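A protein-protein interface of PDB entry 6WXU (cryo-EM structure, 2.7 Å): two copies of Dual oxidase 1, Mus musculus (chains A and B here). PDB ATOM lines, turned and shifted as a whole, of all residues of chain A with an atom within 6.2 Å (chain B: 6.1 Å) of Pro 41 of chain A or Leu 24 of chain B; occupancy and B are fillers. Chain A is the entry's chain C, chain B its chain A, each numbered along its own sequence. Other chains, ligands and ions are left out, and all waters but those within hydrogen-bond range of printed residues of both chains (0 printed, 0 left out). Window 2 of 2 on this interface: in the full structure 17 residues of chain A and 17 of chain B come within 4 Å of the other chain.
The guanidinium group (NH1) of Arg 35 of chain A sits at hydrogen-bond distance from the backbone carbonyl oxygen (O) of Met 25 of chain B (3.0 Å).
The guanidinium group of Arg 38 of chain A is in hydrogen-bond range of the backbone carbonyl oxygen of Gly 416 of chain A (3.3 Å).
Among the printed residues, merely in contact across the chains: Arg 38 of chain A with Met 25 of chain B (3.7 Å), Pro 41 of chain A with Leu 24 of chain B (3.8 Å), Val 40 of chain A with Leu 24 of chain B (3.95 Å) and Leu 39 of chain A with Leu 24 of chain B (3.98 Å).
Of chain B, only Leu 24 comes within 4 Å of Pro 41 of chain A.
Leu 24 of chain B touches just these residues of chain A: Leu 39 (3.98 Å), Val 40 (3.95 Å) and Pro 41 (3.8 Å).
Of the printed residues of chain B, Arg 35 of chain A touches Met 25 (3.0 Å).
Printed residues of chain B within 4 Å of Leu 39 of chain A: Leu 24.
Of the printed residues of chain B, Arg 38 of chain A touches Met 25.
Of the printed residues of chain B, Val 40 of chain A touches Leu 24 (3.95 Å).
Printed residues of chain A within 4 Å of Met 25 of chain B: Arg 35 (3.0 Å) and Arg 38 (3.7 Å).
The nearest printed residue of chain B that does not touch Pro 41 of chain A is Arg 498 of chain B (8.2 Å).
Printed residues of chain A that touch a printed residue of chain B: Arg 35, Arg 38, Leu 39, Val 40 and Pro 41.
Hydrophobic or aromatic side chains of chain A that line the printed part of chain B: Pro 41.
Hydrophobic or aromatic side chains of chain B within 4 Å of the printed part of chain A: Leu 24 and Met 25.
Among the printed residues, 5 pairs touch across the chains.
Among the printed residues, no Asp or Glu carboxylate lies within 4 Å of a Lys or Arg side-chain nitrogen of the other chain.
No position is printed for both chains.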
ATOM      1  N   ARG A  35      28.376  -0.002   2.126  1.00  0.00           N
ATOM      2  CA  ARG A  35      27.394   0.944   2.626  1.00  0.00           C
ATOM      3  C   ARG A  35      26.371   0.262   3.525  1.00  0.00           C
ATOM      4  O   ARG A  35      26.122  -0.939   3.433  1.00  0.00           O
ATOM      5  CB  ARG A  35      26.659   1.611   1.467  1.00  0.00           C
ATOM      6  CG  ARG A  35      27.363   2.785   0.860  1.00  0.00           C
ATOM      7  CD  ARG A  35      26.747   3.159  -0.477  1.00  0.00           C
ATOM      8  NE  ARG A  35      25.291   3.193  -0.435  1.00  0.00           N
ATOM      9  CZ  ARG A  35      24.508   2.355  -1.104  1.00  0.00           C
ATOM     10  NH1 ARG A  35      23.193   2.458  -1.006  1.00  0.00           N
ATOM     11  NH2 ARG A  35      25.040   1.422  -1.877  1.00  0.00           N
ATOM     12  N   ARG A  38      19.621   2.230   3.957  1.00  0.00           N
ATOM     13  CA  ARG A  38      18.592   2.660   4.887  1.00  0.00           C
ATOM     14  C   ARG A  38      17.195   2.336   4.371  1.00  0.00           C
ATOM     15  O   ARG A  38      16.985   2.059   3.190  1.00  0.00           O
ATOM     16  CB  ARG A  38      18.717   4.158   5.150  1.00  0.00           C
ATOM     17  CG  ARG A  38      18.964   4.959   3.897  1.00  0.00           C
ATOM     18  CD  ARG A  38      19.051   6.442   4.177  1.00  0.00           C
ATOM     19  NE  ARG A  38      20.343   6.852   4.714  1.00  0.00           N
ATOM     20  CZ  ARG A  38      20.554   7.168   5.983  1.00  0.00           C
ATOM     21  NH1 ARG A  38      19.558   7.117   6.851  1.00  0.00           N
ATOM     22  NH2 ARG A  38      21.759   7.538   6.386  1.00  0.00           N
ATOM     23  N   LEU A  39      16.230   2.384   5.287  1.00  0.00           N
ATOM     24  CA  LEU A  39      14.839   2.090   4.979  1.00  0.00           C
ATOM     25  C   LEU A  39      14.011   3.334   4.706  1.00  0.00           C
ATOM     26  O   LEU A  39      13.039   3.266   3.947  1.00  0.00           O
ATOM     27  CB  LEU A  39      14.194   1.316   6.131  1.00  0.00           C
ATOM     28  CG  LEU A  39      14.976   0.142   6.715  1.00  0.00           C
ATOM     29  CD1 LEU A  39      14.188  -0.502   7.831  1.00  0.00           C
ATOM     30  CD2 LEU A  39      15.292  -0.869   5.640  1.00  0.00           C
ATOM     31  N   VAL A  40      14.367   4.460   5.314  1.00  0.00           N
ATOM     32  CA  VAL A  40      13.684   5.735   5.120  1.00  0.00           C
ATOM     33  C   VAL A  40      14.733   6.729   4.636  1.00  0.00           C
ATOM     34  O   VAL A  40      15.890   6.639   5.064  1.00  0.00           O
ATOM     35  CB  VAL A  40      13.008   6.199   6.420  1.00  0.00           C
ATOM     36  CG1 VAL A  40      12.054   7.334   6.160  1.00  0.00           C
ATOM     37  CG2 VAL A  40      12.275   5.053   7.079  1.00  0.00           C
ATOM     38  N   PRO A  41      14.400   7.662   3.742  1.00  0.00           N
ATOM     39  CA  PRO A  41      15.389   8.656   3.313  1.00  0.00           C
ATOM     40  C   PRO A  41      16.011   9.399   4.489  1.00  0.00           C
ATOM     41  O   PRO A  41      15.370   9.629   5.514  1.00  0.00           O
ATOM     42  CB  PRO A  41      14.571   9.598   2.426  1.00  0.00           C
ATOM     43  CG  PRO A  41      13.526   8.733   1.860  1.00  0.00           C
ATOM     44  CD  PRO A  41      13.177   7.731   2.924  1.00  0.00           C
ATOM     45  N   ALA A  42      17.273   9.788   4.317  1.00  0.00           N
ATOM     46  CA  ALA A  42      18.042  10.374   5.407  1.00  0.00           C
ATOM     47  C   ALA A  42      17.441  11.698   5.846  1.00  0.00           C
ATOM     48  O   ALA A  42      17.090  12.541   5.016  1.00  0.00           O
ATOM     49  CB  ALA A  42      19.491  10.578   4.976  1.00  0.00           C
ATOM     50  N   SER A  43      17.329  11.885   7.154  1.00  0.00           N
ATOM     51  CA  SER A  43      16.782  13.110   7.725  1.00  0.00           C
ATOM     52  C   SER A  43      17.925  13.869   8.389  1.00  0.00           C
ATOM     53  O   SER A  43      18.180  13.721   9.583  1.00  0.00           O
ATOM     54  CB  SER A  43      15.667  12.809   8.708  1.00  0.00           C
ATOM     55  OG  SER A  43      16.188  12.341   9.930  1.00  0.00           O
ATOM     56  N   PRO A 147      22.154  11.530  -0.043  1.00  0.00           N
ATOM     57  CA  PRO A 147      22.748  11.922   1.239  1.00  0.00           C
ATOM     58  C   PRO A 147      23.779  10.933   1.754  1.00  0.00           C
ATOM     59  O   PRO A 147      23.986   9.877   1.155  1.00  0.00           O
ATOM     60  CB  PRO A 147      21.536  11.996   2.172  1.00  0.00           C
ATOM     61  CG  PRO A 147      20.378  12.158   1.273  1.00  0.00           C
ATOM     62  CD  PRO A 147      20.703  11.346   0.077  1.00  0.00           C
ATOM     63  N   GLY A 416      21.646  10.044  10.670  1.00  0.00           N
ATOM     64  CA  GLY A 416      20.507  10.542   9.927  1.00  0.00           C
ATOM     65  C   GLY A 416      19.295   9.647  10.029  1.00  0.00           C
ATOM     66  O   GLY A 416      18.628   9.397   9.023  1.00  0.00           O
ATOM     67  N   LEU A 417      19.000   9.159  11.208  1.00  0.00           N
ATOM     68  CA  LEU A 417      17.912   8.215  11.362  1.00  0.00           C
ATOM     69  C   LEU A 417      16.569   8.934  11.376  1.00  0.00           C
ATOM     70  O   LEU A 417      16.482  10.090  11.788  1.00  0.00           O
ATOM     71  CB  LEU A 417      18.079   7.421  12.647  1.00  0.00           C
ATOM     72  CG  LEU A 417      19.252   6.456  12.655  1.00  0.00           C
ATOM     73  CD1 LEU A 417      19.259   5.708  13.943  1.00  0.00           C
ATOM     74  CD2 LEU A 417      19.119   5.507  11.508  1.00  0.00           C
ATOM     75  N   PRO A 418      15.507   8.266  10.936  1.00  0.00           N
ATOM     76  CA  PRO A 418      14.193   8.906  10.914  1.00  0.00           C
ATOM     77  C   PRO A 418      13.644   9.095  12.316  1.00  0.00           C
ATOM     78  O   PRO A 418      14.200   8.633  13.312  1.00  0.00           O
ATOM     79  CB  PRO A 418      13.344   7.921  10.113  1.00  0.00           C
ATOM     80  CG  PRO A 418      13.974   6.623  10.362  1.00  0.00           C
ATOM     81  CD  PRO A 418      15.442   6.892  10.417  1.00  0.00           C
ATOM     82  N   LYS A 422       7.790   8.619  11.851  1.00  0.00           N
ATOM     83  CA  LYS A 422       8.106   8.500  10.436  1.00  0.00           C
ATOM     84  C   LYS A 422       8.609   7.107  10.095  1.00  0.00           C
ATOM     85  O   LYS A 422       8.298   6.578   9.024  1.00  0.00           O
ATOM     86  CB  LYS A 422       9.138   9.550  10.040  1.00  0.00           C
ATOM     87  CG  LYS A 422       9.649   9.394   8.627  1.00  0.00           C
ATOM     88  CD  LYS A 422       9.699  10.724   7.908  1.00  0.00           C
ATOM     89  CE  LYS A 422      10.541  11.726   8.669  1.00  0.00           C
ATOM     90  NZ  LYS A 422      11.934  11.245   8.847  1.00  0.00           N
ATOM     91  N   TYR B  21      17.109   6.674  -9.870  1.00  0.00           N
ATOM     92  CA  TYR B  21      16.498   7.074  -8.603  1.00  0.00           C
ATOM     93  C   TYR B  21      15.091   6.520  -8.440  1.00  0.00           C
ATOM     94  O   TYR B  21      14.238   7.144  -7.810  1.00  0.00           O
ATOM     95  CB  TYR B  21      16.489   8.595  -8.445  1.00  0.00           C
ATOM     96  CG  TYR B  21      17.850   9.214  -8.592  1.00  0.00           C
ATOM     97  CD1 TYR B  21      18.834   8.994  -7.648  1.00  0.00           C
ATOM     98  CD2 TYR B  21      18.155  10.015  -9.676  1.00  0.00           C
ATOM     99  CE1 TYR B  21      20.079   9.550  -7.778  1.00  0.00           C
ATOM    100  CE2 TYR B  21      19.396  10.577  -9.815  1.00  0.00           C
ATOM    101  CZ  TYR B  21      20.354  10.340  -8.864  1.00  0.00           C
ATOM    102  OH  TYR B  21      21.599  10.899  -8.995  1.00  0.00           O
ATOM    103  N   ASN B  22      14.830   5.348  -9.011  1.00  0.00           N
ATOM    104  CA  ASN B  22      13.571   4.671  -8.739  1.00  0.00           C
ATOM    105  C   ASN B  22      13.633   3.908  -7.428  1.00  0.00           C
ATOM    106  O   ASN B  22      12.615   3.773  -6.746  1.00  0.00           O
ATOM    107  CB  ASN B  22      13.221   3.723  -9.883  1.00  0.00           C
ATOM    108  CG  ASN B  22      11.796   3.236  -9.819  1.00  0.00           C
ATOM    109  OD1 ASN B  22      11.425   2.483  -8.928  1.00  0.00           O
ATOM    110  ND2 ASN B  22      10.989   3.654 -10.777  1.00  0.00           N
ATOM    111  N   ASN B  23      14.809   3.413  -7.064  1.00  0.00           N
ATOM    112  CA  ASN B  23      15.026   2.698  -5.818  1.00  0.00           C
ATOM    113  C   ASN B  23      15.816   3.581  -4.865  1.00  0.00           C
ATOM    114  O   ASN B  23      16.734   4.290  -5.281  1.00  0.00           O
ATOM    115  CB  ASN B  23      15.780   1.395  -6.066  1.00  0.00           C
ATOM    116  CG  ASN B  23      15.405   0.319  -5.088  1.00  0.00           C
ATOM    117  OD1 ASN B  23      14.232   0.028  -4.899  1.00  0.00           O
ATOM    118  ND2 ASN B  23      16.396  -0.272  -4.448  1.00  0.00           N
ATOM    119  N   LEU B  24      15.460   3.537  -3.584  1.00  0.00           N
ATOM    120  CA  LEU B  24      16.140   4.394  -2.620  1.00  0.00           C
ATOM    121  C   LEU B  24      17.579   3.951  -2.398  1.00  0.00           C
ATOM    122  O   LEU B  24      18.479   4.788  -2.280  1.00  0.00           O
ATOM    123  CB  LEU B  24      15.372   4.413  -1.303  1.00  0.00           C
ATOM    124  CG  LEU B  24      16.033   5.124  -0.126  1.00  0.00           C
ATOM    125  CD1 LEU B  24      16.348   6.555  -0.472  1.00  0.00           C
ATOM    126  CD2 LEU B  24      15.131   5.060   1.076  1.00  0.00           C
ATOM    127  N   MET B  25      17.821   2.645  -2.358  1.00  0.00           N
ATOM    128  CA  MET B  25      19.134   2.127  -2.006  1.00  0.00           C
ATOM    129  C   MET B  25      20.030   1.944  -3.224  1.00  0.00           C
ATOM    130  O   MET B  25      21.176   2.397  -3.224  1.00  0.00           O
ATOM    131  CB  MET B  25      18.972   0.806  -1.264  1.00  0.00           C
ATOM    132  CG  MET B  25      17.875   0.839  -0.225  1.00  0.00           C
ATOM    133  SD  MET B  25      17.515  -0.792   0.424  1.00  0.00           S
ATOM    134  CE  MET B  25      17.388  -1.715  -1.101  1.00  0.00           C
ATOM    135  N   GLU B  26      19.532   1.289  -4.265  1.00  0.00           N
ATOM    136  CA  GLU B  26      20.286   1.079  -5.496  1.00  0.00           C
ATOM    137  C   GLU B  26      19.741   2.035  -6.548  1.00  0.00           C
ATOM    138  O   GLU B  26      18.726   1.755  -7.187  1.00  0.00           O
ATOM    139  CB  GLU B  26      20.179  -0.372  -5.944  1.00  0.00           C
ATOM    140  CG  GLU B  26      20.587  -1.376  -4.882  1.00  0.00           C
ATOM    141  CD  GLU B  26      22.084  -1.559  -4.800  1.00  0.00           C
ATOM    142  OE1 GLU B  26      22.790  -1.090  -5.712  1.00  0.00           O
ATOM    143  OE2 GLU B  26      22.557  -2.177  -3.826  1.00  0.00           O
ATOM    144  N   HIS B  27      20.423   3.165  -6.734  1.00  0.00           N
ATOM    145  CA  HIS B  27      19.922   4.191  -7.641  1.00  0.00           C
ATOM    146  C   HIS B  27      19.968   3.743  -9.090  1.00  0.00           C
ATOM    147  O   HIS B  27      19.159   4.198  -9.902  1.00  0.00           O
ATOM    148  CB  HIS B  27      20.729   5.474  -7.486  1.00  0.00           C
ATOM    149  CG  HIS B  27      20.573   6.132  -6.153  1.00  0.00           C
ATOM    150  ND1 HIS B  27      19.395   6.098  -5.442  1.00  0.00           N
ATOM    151  CD2 HIS B  27      21.446   6.842  -5.404  1.00  0.00           C
ATOM    152  CE1 HIS B  27      19.550   6.759  -4.310  1.00  0.00           C
ATOM    153  NE2 HIS B  27      20.786   7.218  -4.261  1.00  0.00           N
ATOM    154  N   TYR B 295       4.890  -2.948  -2.227  1.00  0.00           N
ATOM    155  CA  TYR B 295       6.192  -2.577  -2.760  1.00  0.00           C
ATOM    156  C   TYR B 295       7.300  -3.214  -1.930  1.00  0.00           C
ATOM    157  O   TYR B 295       7.368  -3.009  -0.714  1.00  0.00           O
ATOM    158  CB  TYR B 295       6.315  -1.059  -2.775  1.00  0.00           C
ATOM    159  CG  TYR B 295       7.666  -0.520  -3.154  1.00  0.00           C
ATOM    160  CD1 TYR B 295       8.343  -1.003  -4.253  1.00  0.00           C
ATOM    161  CD2 TYR B 295       8.253   0.489  -2.419  1.00  0.00           C
ATOM    162  CE1 TYR B 295       9.571  -0.508  -4.596  1.00  0.00           C
ATOM    163  CE2 TYR B 295       9.478   0.988  -2.758  1.00  0.00           C
ATOM    164  CZ  TYR B 295      10.134   0.485  -3.847  1.00  0.00           C
ATOM    165  OH  TYR B 295      11.363   0.980  -4.193  1.00  0.00           O
ATOM    166  N   ARG B 498       8.842   1.200  -7.712  1.00  0.00           N
ATOM    167  CA  ARG B 498       8.203   2.141  -6.802  1.00  0.00           C
ATOM    168  C   ARG B 498       6.985   2.788  -7.433  1.00  0.00           C
ATOM    169  O   ARG B 498       6.011   3.088  -6.736  1.00  0.00           O
ATOM    170  CB  ARG B 498       9.198   3.213  -6.367  1.00  0.00           C
ATOM    171  CG  ARG B 498       8.606   4.295  -5.496  1.00  0.00           C
ATOM    172  CD  ARG B 498       9.665   4.979  -4.665  1.00  0.00           C
ATOM    173  NE  ARG B 498      10.631   5.702  -5.479  1.00  0.00           N
ATOM    174  CZ  ARG B 498      10.560   7.001  -5.742  1.00  0.00           C
ATOM    175  NH1 ARG B 498       9.565   7.722  -5.256  1.00  0.00           N
ATOM    176  NH2 ARG B 498      11.487   7.578  -6.487  1.00  0.00           N
